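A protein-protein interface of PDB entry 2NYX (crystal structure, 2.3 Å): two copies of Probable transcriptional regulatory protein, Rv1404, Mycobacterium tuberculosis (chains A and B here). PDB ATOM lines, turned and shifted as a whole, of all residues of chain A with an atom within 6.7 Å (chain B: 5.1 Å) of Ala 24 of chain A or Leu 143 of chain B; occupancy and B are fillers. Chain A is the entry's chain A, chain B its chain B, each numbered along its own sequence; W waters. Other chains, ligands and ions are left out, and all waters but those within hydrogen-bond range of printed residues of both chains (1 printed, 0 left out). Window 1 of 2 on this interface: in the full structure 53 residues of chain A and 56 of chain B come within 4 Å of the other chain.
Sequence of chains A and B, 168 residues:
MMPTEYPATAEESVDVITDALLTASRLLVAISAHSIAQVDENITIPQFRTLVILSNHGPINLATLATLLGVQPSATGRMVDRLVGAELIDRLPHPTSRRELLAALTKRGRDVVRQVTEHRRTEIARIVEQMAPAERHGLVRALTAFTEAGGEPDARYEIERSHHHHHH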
ATOM      1  N   VAL A  16       0.449  -1.975  34.479  1.00  0.00           N
ATOM      2  CA  VAL A  16       0.253  -0.839  33.556  1.00  0.00           C
ATOM      3  C   VAL A  16       0.835  -1.060  32.158  1.00  0.00           C
ATOM      4  O   VAL A  16       0.286  -0.541  31.177  1.00  0.00           O
ATOM      5  CB  VAL A  16       0.753   0.531  34.122  1.00  0.00           C
ATOM      6  CG1 VAL A  16      -0.152   1.009  35.264  1.00  0.00           C
ATOM      7  CG2 VAL A  16       2.212   0.468  34.555  1.00  0.00           C
ATOM      8  N   ILE A  17       1.936  -1.814  32.075  1.00  0.00           N
ATOM      9  CA  ILE A  17       2.527  -2.187  30.784  1.00  0.00           C
ATOM     10  C   ILE A  17       1.600  -3.149  30.045  1.00  0.00           C
ATOM     11  O   ILE A  17       1.350  -2.990  28.858  1.00  0.00           O
ATOM     12  CB  ILE A  17       3.961  -2.792  30.930  1.00  0.00           C
ATOM     13  CG1 ILE A  17       4.938  -1.750  31.496  1.00  0.00           C
ATOM     14  CG2 ILE A  17       4.491  -3.290  29.588  1.00  0.00           C
ATOM     15  CD1 ILE A  17       6.245  -2.340  32.031  1.00  0.00           C
ATOM     16  N   THR A  18       1.089  -4.136  30.766  1.00  0.00           N
ATOM     17  CA  THR A  18       0.163  -5.129  30.230  1.00  0.00           C
ATOM     18  C   THR A  18      -1.135  -4.483  29.737  1.00  0.00           C
ATOM     19  O   THR A  18      -1.568  -4.750  28.620  1.00  0.00           O
ATOM     20  CB  THR A  18      -0.124  -6.227  31.297  1.00  0.00           C
ATOM     21  OG1 THR A  18       1.105  -6.871  31.660  1.00  0.00           O
ATOM     22  CG2 THR A  18      -1.099  -7.269  30.792  1.00  0.00           C
ATOM     23  N   ASP A  19      -1.745  -3.632  30.564  1.00  0.00           N
ATOM     24  CA  ASP A  19      -2.973  -2.939  30.187  1.00  0.00           C
ATOM     25  C   ASP A  19      -2.781  -2.131  28.895  1.00  0.00           C
ATOM     26  O   ASP A  19      -3.627  -2.160  28.005  1.00  0.00           O
ATOM     27  CB  ASP A  19      -3.472  -2.045  31.334  1.00  0.00           C
ATOM     28  CG  ASP A  19      -3.927  -2.846  32.583  1.00  0.00           C
ATOM     29  OD1 ASP A  19      -4.323  -4.035  32.468  1.00  0.00           O
ATOM     30  OD2 ASP A  19      -3.902  -2.278  33.701  1.00  0.00           O
ATOM     31  N   ALA A  20      -1.651  -1.436  28.780  1.00  0.00           N
ATOM     32  CA  ALA A  20      -1.369  -0.623  27.599  1.00  0.00           C
ATOM     33  C   ALA A  20      -1.179  -1.487  26.348  1.00  0.00           C
ATOM     34  O   ALA A  20      -1.625  -1.131  25.249  1.00  0.00           O
ATOM     35  CB  ALA A  20      -0.154   0.242  27.845  1.00  0.00           C
ATOM     36  N   LEU A  21      -0.516  -2.628  26.533  1.00  0.00           N
ATOM     37  CA  LEU A  21      -0.326  -3.619  25.479  1.00  0.00           C
ATOM     38  C   LEU A  21      -1.635  -4.296  25.068  1.00  0.00           C
ATOM     39  O   LEU A  21      -1.843  -4.593  23.889  1.00  0.00           O
ATOM     40  CB  LEU A  21       0.703  -4.661  25.916  1.00  0.00           C
ATOM     41  CG  LEU A  21       2.165  -4.266  25.746  1.00  0.00           C
ATOM     42  CD1 LEU A  21       3.010  -5.083  26.666  1.00  0.00           C
ATOM     43  CD2 LEU A  21       2.615  -4.445  24.322  1.00  0.00           C
ATOM     44  N   LEU A  22      -2.518  -4.508  26.041  1.00  0.00           N
ATOM     45  CA  LEU A  22      -3.839  -5.063  25.777  1.00  0.00           C
ATOM     46  C   LEU A  22      -4.672  -4.169  24.851  1.00  0.00           C
ATOM     47  O   LEU A  22      -5.231  -4.648  23.868  1.00  0.00           O
ATOM     48  CB  LEU A  22      -4.581  -5.343  27.078  1.00  0.00           C
ATOM     49  CG  LEU A  22      -5.925  -6.059  26.983  1.00  0.00           C
ATOM     50  CD1 LEU A  22      -5.834  -7.409  26.230  1.00  0.00           C
ATOM     51  CD2 LEU A  22      -6.498  -6.266  28.380  1.00  0.00           C
ATOM     52  N   THR A  23      -4.741  -2.877  25.150  1.00  0.00           N
ATOM     53  CA  THR A  23      -5.453  -1.956  24.291  1.00  0.00           C
ATOM     54  C   THR A  23      -4.782  -1.880  22.915  1.00  0.00           C
ATOM     55  O   THR A  23      -5.476  -1.899  21.890  1.00  0.00           O
ATOM     56  CB  THR A  23      -5.575  -0.572  24.928  1.00  0.00           C
ATOM     57  OG1 THR A  23      -6.098  -0.702  26.259  1.00  0.00           O
ATOM     58  CG2 THR A  23      -6.513   0.296  24.123  1.00  0.00           C
ATOM     59  N   ALA A  24      -3.446  -1.826  22.886  1.00  0.00           N
ATOM     60  CA  ALA A  24      -2.707  -1.865  21.617  1.00  0.00           C
ATOM     61  C   ALA A  24      -3.033  -3.102  20.792  1.00  0.00           C
ATOM     62  O   ALA A  24      -3.118  -3.020  19.568  1.00  0.00           O
ATOM     63  CB  ALA A  24      -1.201  -1.776  21.847  1.00  0.00           C
ATOM     64  N   SER A  25      -3.217  -4.237  21.462  1.00  0.00           N
ATOM     65  CA  SER A  25      -3.541  -5.491  20.781  1.00  0.00           C
ATOM     66  C   SER A  25      -4.920  -5.450  20.110  1.00  0.00           C
ATOM     67  O   SER A  25      -5.113  -6.044  19.039  1.00  0.00           O
ATOM     68  CB  SER A  25      -3.442  -6.673  21.742  1.00  0.00           C
ATOM     69  OG  SER A  25      -4.538  -6.682  22.625  1.00  0.00           O
ATOM     70  N   ARG A  26      -5.864  -4.745  20.741  1.00  0.00           N
ATOM     71  CA  ARG A  26      -7.180  -4.506  20.167  1.00  0.00           C
ATOM     72  C   ARG A  26      -7.119  -3.633  18.924  1.00  0.00           C
ATOM     73  O   ARG A  26      -7.877  -3.848  17.972  1.00  0.00           O
ATOM     74  CB  ARG A  26      -8.103  -3.853  21.183  1.00  0.00           C
ATOM     75  CG  ARG A  26      -8.630  -4.809  22.201  1.00  0.00           C
ATOM     76  CD  ARG A  26      -9.801  -4.221  22.923  1.00  0.00           C
ATOM     77  NE  ARG A  26     -10.439  -5.221  23.760  1.00  0.00           N
ATOM     78  CZ  ARG A  26     -11.490  -4.988  24.526  1.00  0.00           C
ATOM     79  NH1 ARG A  26     -12.019  -3.780  24.558  1.00  0.00           N
ATOM     80  NH2 ARG A  26     -12.005  -5.960  25.264  1.00  0.00           N
ATOM     81  N   LEU A  27      -6.228  -2.646  18.926  1.00  0.00           N
ATOM     82  CA  LEU A  27      -6.085  -1.780  17.764  1.00  0.00           C
ATOM     83  C   LEU A  27      -5.445  -2.541  16.601  1.00  0.00           C
ATOM     84  O   LEU A  27      -5.781  -2.296  15.453  1.00  0.00           O
ATOM     85  CB  LEU A  27      -5.321  -0.497  18.112  1.00  0.00           C
ATOM     86  CG  LEU A  27      -5.037   0.587  17.063  1.00  0.00           C
ATOM     87  CD1 LEU A  27      -6.280   1.068  16.307  1.00  0.00           C
ATOM     88  CD2 LEU A  27      -4.365   1.768  17.729  1.00  0.00           C
ATOM     89  N   LEU A  28      -4.552  -3.481  16.891  1.00  0.00           N
ATOM     90  CA  LEU A  28      -3.933  -4.260  15.822  1.00  0.00           C
ATOM     91  C   LEU A  28      -4.911  -5.270  15.234  1.00  0.00           C
ATOM     92  O   LEU A  28      -4.921  -5.503  14.013  1.00  0.00           O
ATOM     93  CB  LEU A  28      -2.652  -4.938  16.296  1.00  0.00           C
ATOM     94  CG  LEU A  28      -1.513  -3.981  16.656  1.00  0.00           C
ATOM     95  CD1 LEU A  28      -0.576  -4.630  17.639  1.00  0.00           C
ATOM     96  CD2 LEU A  28      -0.754  -3.518  15.428  1.00  0.00           C
ATOM     97  N   VAL A  29      -5.750  -5.846  16.091  1.00  0.00           N
ATOM     98  CA  VAL A  29      -6.851  -6.698  15.621  1.00  0.00           C
ATOM     99  C   VAL A  29      -7.823  -5.919  14.737  1.00  0.00           C
ATOM    100  O   VAL A  29      -8.227  -6.404  13.677  1.00  0.00           O
ATOM    101  CB  VAL A  29      -7.595  -7.396  16.772  1.00  0.00           C
ATOM    102  CG1 VAL A  29      -8.880  -8.009  16.272  1.00  0.00           C
ATOM    103  CG2 VAL A  29      -6.729  -8.478  17.370  1.00  0.00           C
ATOM    104  N   MET A 131       0.723  10.498  14.991  1.00  0.00           N
ATOM    105  CA  MET A 131       1.633  10.499  16.128  1.00  0.00           C
ATOM    106  C   MET A 131       2.844  11.375  15.885  1.00  0.00           C
ATOM    107  O   MET A 131       3.330  11.494  14.751  1.00  0.00           O
ATOM    108  CB  MET A 131       2.112   9.088  16.426  1.00  0.00           C
ATOM    109  CG  MET A 131       1.023   8.124  16.800  1.00  0.00           C
ATOM    110  SD  MET A 131       1.691   6.304  16.612  1.00  0.00           S
ATOM    111  CE  MET A 131       2.737   6.125  18.349  1.00  0.00           C
ATOM    112  N   GLU A 135       6.974   9.520  19.419  1.00  0.00           N
ATOM    113  CA  GLU A 135       6.027   8.491  19.849  1.00  0.00           C
ATOM    114  C   GLU A 135       6.102   7.297  18.903  1.00  0.00           C
ATOM    115  O   GLU A 135       6.077   6.148  19.334  1.00  0.00           O
ATOM    116  CB  GLU A 135       4.599   9.035  19.882  1.00  0.00           C
ATOM    117  CG  GLU A 135       4.325  10.129  20.911  1.00  0.00           C
ATOM    118  CD  GLU A 135       3.078  10.972  20.561  1.00  0.00           C
ATOM    119  OE1 GLU A 135       2.376  10.658  19.562  1.00  0.00           O
ATOM    120  OE2 GLU A 135       2.793  11.957  21.289  1.00  0.00           O
ATOM    121  N   GLY A 138       9.170   5.384  19.828  1.00  0.00           N
ATOM    122  CA  GLY A 138       8.896   4.735  21.098  1.00  0.00           C
ATOM    123  C   GLY A 138       8.014   3.507  20.962  1.00  0.00           C
ATOM    124  O   GLY A 138       8.146   2.558  21.738  1.00  0.00           O
ATOM    125  N   LEU A 139       7.119   3.531  19.974  1.00  0.00           N
ATOM    126  CA  LEU A 139       6.195   2.429  19.712  1.00  0.00           C
ATOM    127  C   LEU A 139       6.911   1.218  19.104  1.00  0.00           C
ATOM    128  O   LEU A 139       6.683   0.088  19.525  1.00  0.00           O
ATOM    129  CB  LEU A 139       5.051   2.919  18.818  1.00  0.00           C
ATOM    130  CG  LEU A 139       3.680   2.238  18.750  1.00  0.00           C
ATOM    131  CD1 LEU A 139       3.486   1.549  17.433  1.00  0.00           C
ATOM    132  CD2 LEU A 139       3.383   1.284  19.916  1.00  0.00           C
ATOM    133  N   ALA A 142       8.796  -0.269  21.963  1.00  0.00           N
ATOM    134  CA  ALA A 142       7.927  -0.958  22.912  1.00  0.00           C
ATOM    135  C   ALA A 142       7.507  -2.346  22.431  1.00  0.00           C
ATOM    136  O   ALA A 142       7.538  -3.309  23.191  1.00  0.00           O
ATOM    137  CB  ALA A 142       6.699  -0.106  23.209  1.00  0.00           C
ATOM    138  N   LEU A 143       7.106  -2.437  21.167  1.00  0.00           N
ATOM    139  CA  LEU A 143       6.636  -3.691  20.590  1.00  0.00           C
ATOM    140  C   LEU A 143       7.783  -4.649  20.269  1.00  0.00           C
ATOM    141  O   LEU A 143       7.597  -5.860  20.246  1.00  0.00           O
ATOM    142  CB  LEU A 143       5.811  -3.417  19.337  1.00  0.00           C
ATOM    143  CG  LEU A 143       4.471  -2.711  19.489  1.00  0.00           C
ATOM    144  CD1 LEU A 143       3.836  -2.613  18.121  1.00  0.00           C
ATOM    145  CD2 LEU A 143       3.523  -3.439  20.437  1.00  0.00           C
ATOM    146  N   LEU B  28       2.443  -9.834  19.050  1.00  0.00           N
ATOM    147  CA  LEU B  28       1.227  -9.382  19.697  1.00  0.00           C
ATOM    148  C   LEU B  28       0.022  -9.863  18.909  1.00  0.00           C
ATOM    149  O   LEU B  28      -0.949 -10.350  19.495  1.00  0.00           O
ATOM    150  CB  LEU B  28       1.181  -7.865  19.817  1.00  0.00           C
ATOM    151  CG  LEU B  28       0.860  -7.289  21.202  1.00  0.00           C
ATOM    152  CD1 LEU B  28       0.269  -5.888  21.084  1.00  0.00           C
ATOM    153  CD2 LEU B  28      -0.031  -8.192  22.057  1.00  0.00           C
ATOM    154  N   LEU B 139       7.421   2.906  28.183  1.00  0.00           N
ATOM    155  CA  LEU B 139       6.594   1.983  27.402  1.00  0.00           C
ATOM    156  C   LEU B 139       5.141   2.443  27.281  1.00  0.00           C
ATOM    157  O   LEU B 139       4.597   2.499  26.168  1.00  0.00           O
ATOM    158  CB  LEU B 139       6.668   0.552  27.955  1.00  0.00           C
ATOM    159  CG  LEU B 139       8.022  -0.176  27.925  1.00  0.00           C
ATOM    160  CD1 LEU B 139       7.972  -1.484  28.685  1.00  0.00           C
ATOM    161  CD2 LEU B 139       8.520  -0.403  26.499  1.00  0.00           C
ATOM    162  N   VAL B 140       4.521   2.779  28.418  1.00  0.00           N
ATOM    163  CA  VAL B 140       3.105   3.167  28.432  1.00  0.00           C
ATOM    164  C   VAL B 140       2.853   4.393  27.558  1.00  0.00           C
ATOM    165  O   VAL B 140       1.979   4.369  26.703  1.00  0.00           O
ATOM    166  CB  VAL B 140       2.551   3.380  29.858  1.00  0.00           C
ATOM    167  CG1 VAL B 140       1.152   3.979  29.809  1.00  0.00           C
ATOM    168  CG2 VAL B 140       2.520   2.068  30.614  1.00  0.00           C
ATOM    169  N   ARG B 141       3.630   5.446  27.766  1.00  0.00           N
ATOM    170  CA  ARG B 141       3.533   6.669  26.972  1.00  0.00           C
ATOM    171  C   ARG B 141       3.379   6.375  25.474  1.00  0.00           C
ATOM    172  O   ARG B 141       2.422   6.826  24.847  1.00  0.00           O
ATOM    173  CB  ARG B 141       4.759   7.553  27.240  1.00  0.00           C
ATOM    174  CG  ARG B 141       4.681   8.962  26.660  1.00  0.00           C
ATOM    175  CD  ARG B 141       5.670   9.904  27.356  1.00  0.00           C
ATOM    176  NE  ARG B 141       7.071   9.635  27.013  1.00  0.00           N
ATOM    177  CZ  ARG B 141       7.928   8.936  27.762  1.00  0.00           C
ATOM    178  NH1 ARG B 141       7.553   8.406  28.922  1.00  0.00           N
ATOM    179  NH2 ARG B 141       9.178   8.765  27.350  1.00  0.00           N
ATOM    180  N   ALA B 142       4.303   5.593  24.920  1.00  0.00           N
ATOM    181  CA  ALA B 142       4.305   5.249  23.493  1.00  0.00           C
ATOM    182  C   ALA B 142       3.092   4.415  23.044  1.00  0.00           C
ATOM    183  O   ALA B 142       2.492   4.685  22.006  1.00  0.00           O
ATOM    184  CB  ALA B 142       5.615   4.549  23.123  1.00  0.00           C
ATOM    185  N   LEU B 143       2.741   3.400  23.825  1.00  0.00           N
ATOM    186  CA  LEU B 143       1.584   2.561  23.532  1.00  0.00           C
ATOM    187  C   LEU B 143       0.270   3.330  23.584  1.00  0.00           C
ATOM    188  O   LEU B 143      -0.604   3.124  22.758  1.00  0.00           O
ATOM    189  CB  LEU B 143       1.538   1.361  24.480  1.00  0.00           C
ATOM    190  CG  LEU B 143       2.600   0.283  24.237  1.00  0.00           C
ATOM    191  CD1 LEU B 143       2.775  -0.564  25.487  1.00  0.00           C
ATOM    192  CD2 LEU B 143       2.260  -0.597  23.041  1.00  0.00           C
ATOM    193  N   THR B 144       0.148   4.213  24.567  1.00  0.00           N
ATOM    194  CA  THR B 144      -1.027   5.062  24.762  1.00  0.00           C
ATOM    195  C   THR B 144      -1.203   6.058  23.603  1.00  0.00           C
ATOM    196  O   THR B 144      -2.329   6.326  23.168  1.00  0.00           O
ATOM    197  CB  THR B 144      -0.916   5.807  26.110  1.00  0.00           C
ATOM    198  OG1 THR B 144      -0.890   4.845  27.169  1.00  0.00           O
ATOM    199  CG2 THR B 144      -2.099   6.730  26.336  1.00  0.00           C
ATOM    200  N   ALA B 145      -0.091   6.595  23.104  1.00  0.00           N
ATOM    201  CA  ALA B 145      -0.104   7.483  21.955  1.00  0.00           C
ATOM    202  C   ALA B 145      -0.583   6.738  20.705  1.00  0.00           C
ATOM    203  O   ALA B 145      -1.309   7.292  19.880  1.00  0.00           O
ATOM    204  CB  ALA B 145       1.273   8.084  21.746  1.00  0.00           C
ATOM    205  N   PHE B 146      -0.195   5.472  20.591  1.00  0.00           N
ATOM    206  CA  PHE B 146      -0.654   4.615  19.504  1.00  0.00           C
ATOM    207  C   PHE B 146      -2.168   4.408  19.526  1.00  0.00           C
ATOM    208  O   PHE B 146      -2.829   4.548  18.497  1.00  0.00           O
ATOM    209  CB  PHE B 146       0.058   3.269  19.566  1.00  0.00           C
ATOM    210  CG  PHE B 146      -0.396   2.288  18.524  1.00  0.00           C
ATOM    211  CD1 PHE B 146      -0.347   2.611  17.167  1.00  0.00           C
ATOM    212  CD2 PHE B 146      -0.838   1.018  18.896  1.00  0.00           C
ATOM    213  CE1 PHE B 146      -0.758   1.669  16.201  1.00  0.00           C
ATOM    214  CE2 PHE B 146      -1.238   0.082  17.945  1.00  0.00           C
ATOM    215  CZ  PHE B 146      -1.199   0.398  16.604  1.00  0.00           C
ATOM    216  N   THR B 147      -2.711   4.086  20.698  1.00  0.00           N
ATOM    217  CA  THR B 147      -4.132   3.770  20.817  1.00  0.00           C
ATOM    218  C   THR B 147      -5.026   5.013  20.742  1.00  0.00           C
ATOM    219  O   THR B 147      -6.116   4.958  20.182  1.00  0.00           O
ATOM    220  CB  THR B 147      -4.446   2.911  22.060  1.00  0.00           C
ATOM    221  OG1 THR B 147      -3.983   3.579  23.239  1.00  0.00           O
ATOM    222  CG2 THR B 147      -3.767   1.568  21.945  1.00  0.00           C
HETATM  223  O   HOH W   1      -2.391   1.538  24.873  1.00  0.00           O
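Hydrophobic or aromatic side chains of chain A within 4 Å of the printed part of chain B: Ile 17, Ala 20, Leu 21, Ala 24, Leu 27, Leu 28, Met 131, Leu 139 and Ala 142. Of the 10 printed residues of chain B, 8 touch a printed residue of chain A. Along chain B the printed residues that touch a printed residue of chain A span positions 28 to 147.
Leu 28 of chain A touches its own counterpart, Leu 28 of chain B. Leu 139 of chain A touches Ala 142 of chain B, and with the chains exchanged Ala 142 of chain A touches Leu 139 of chain B. Leu 139 of chain A touches Leu 143 of chain B, but with the chains exchanged Leu 143 of chain A does not touch Leu 139 of chain B (5.9 Å). Positions printed for both chains: 28, 139, 142 and 143.
CD1 of Ile 17 of chain A touches CD1 of Leu 139 of chain B (3.9 Å). Ala 20 of chain A touches Leu 143 of chain B (CB to CD1, 3.8 Å). Thr 23 of chain A touches Thr 147 of chain B. CE2 of Phe 146 of chain B touches O of Ala 24 of chain A, at 3.97 Å. Thr 147 of chain B touches Ala 24 of chain A (CG2 to N, 3.5 Å). Leu 27 of chain A touches Thr 147 of chain B. CD1 of Leu 28 of chain B touches CD1 of Leu 28 of chain A, at 3.8 Å. O of Ala 145 of chain B touches CG of Met 131 of chain A, at 3.95 Å. Gly 138 of chain A touches Ala 142 of chain B (C to CB, 3.4 Å). CD2 of Leu 139 of chain B touches CA of Ala 142 of chain A, at 3.7 Å.
Water W1 lies within hydrogen-bond range of the backbone carbonyl oxygen of Ala 20 of chain A (2.8 Å), the side-chain hydroxyl of Thr 147 of chain B (3.1 Å) and the backbone carbonyl oxygen of Leu 143 of chain B (3.2 Å).
O of Asp 19 of chain A lies within hydrogen-bond range of OG1 of Thr 23 of chain A (3.4 Å). The backbone carbonyl oxygen of Leu 22 of chain A lies within hydrogen-bond range of the side-chain hydroxyl of Ser 25 of chain A, 2.5 Å away. OG1 of Thr 144 of chain B sits at hydrogen-bond distance from O of Val 140 of chain B (2.9 Å). The side-chain hydroxyl of Thr 147 of chain B lies within hydrogen-bond range of the backbone carbonyl oxygen of Leu 143 of chain B, at 3.4 Å. O of Thr 144 of chain B lies within hydrogen-bond range of OG1 of Thr 147 of chain B (3.2 Å).
Of chain B, only Leu 143, Phe 146 and Thr 147 come within 4 Å of Ala 24 of chain A. Printed residues of chain B within 4 Å of Thr 23 of chain A: Thr 147. Of the printed residues of chain B, Leu 28 of chain A touches Leu 28. Of the printed residues of chain A, Val 140 of chain B touches Val 16. Leu 143 of chain A touches none of the printed residues of chain B. Arg 141 of chain B touches none of the printed residues of chain A. The nearest residue of chain A that does not touch Leu 143 of chain B is Leu 143 of chain A (4.1 Å). The nearest printed residue of chain B that does not touch Ala 20 of chain A is Val 140 of chain B (4.3 Å).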
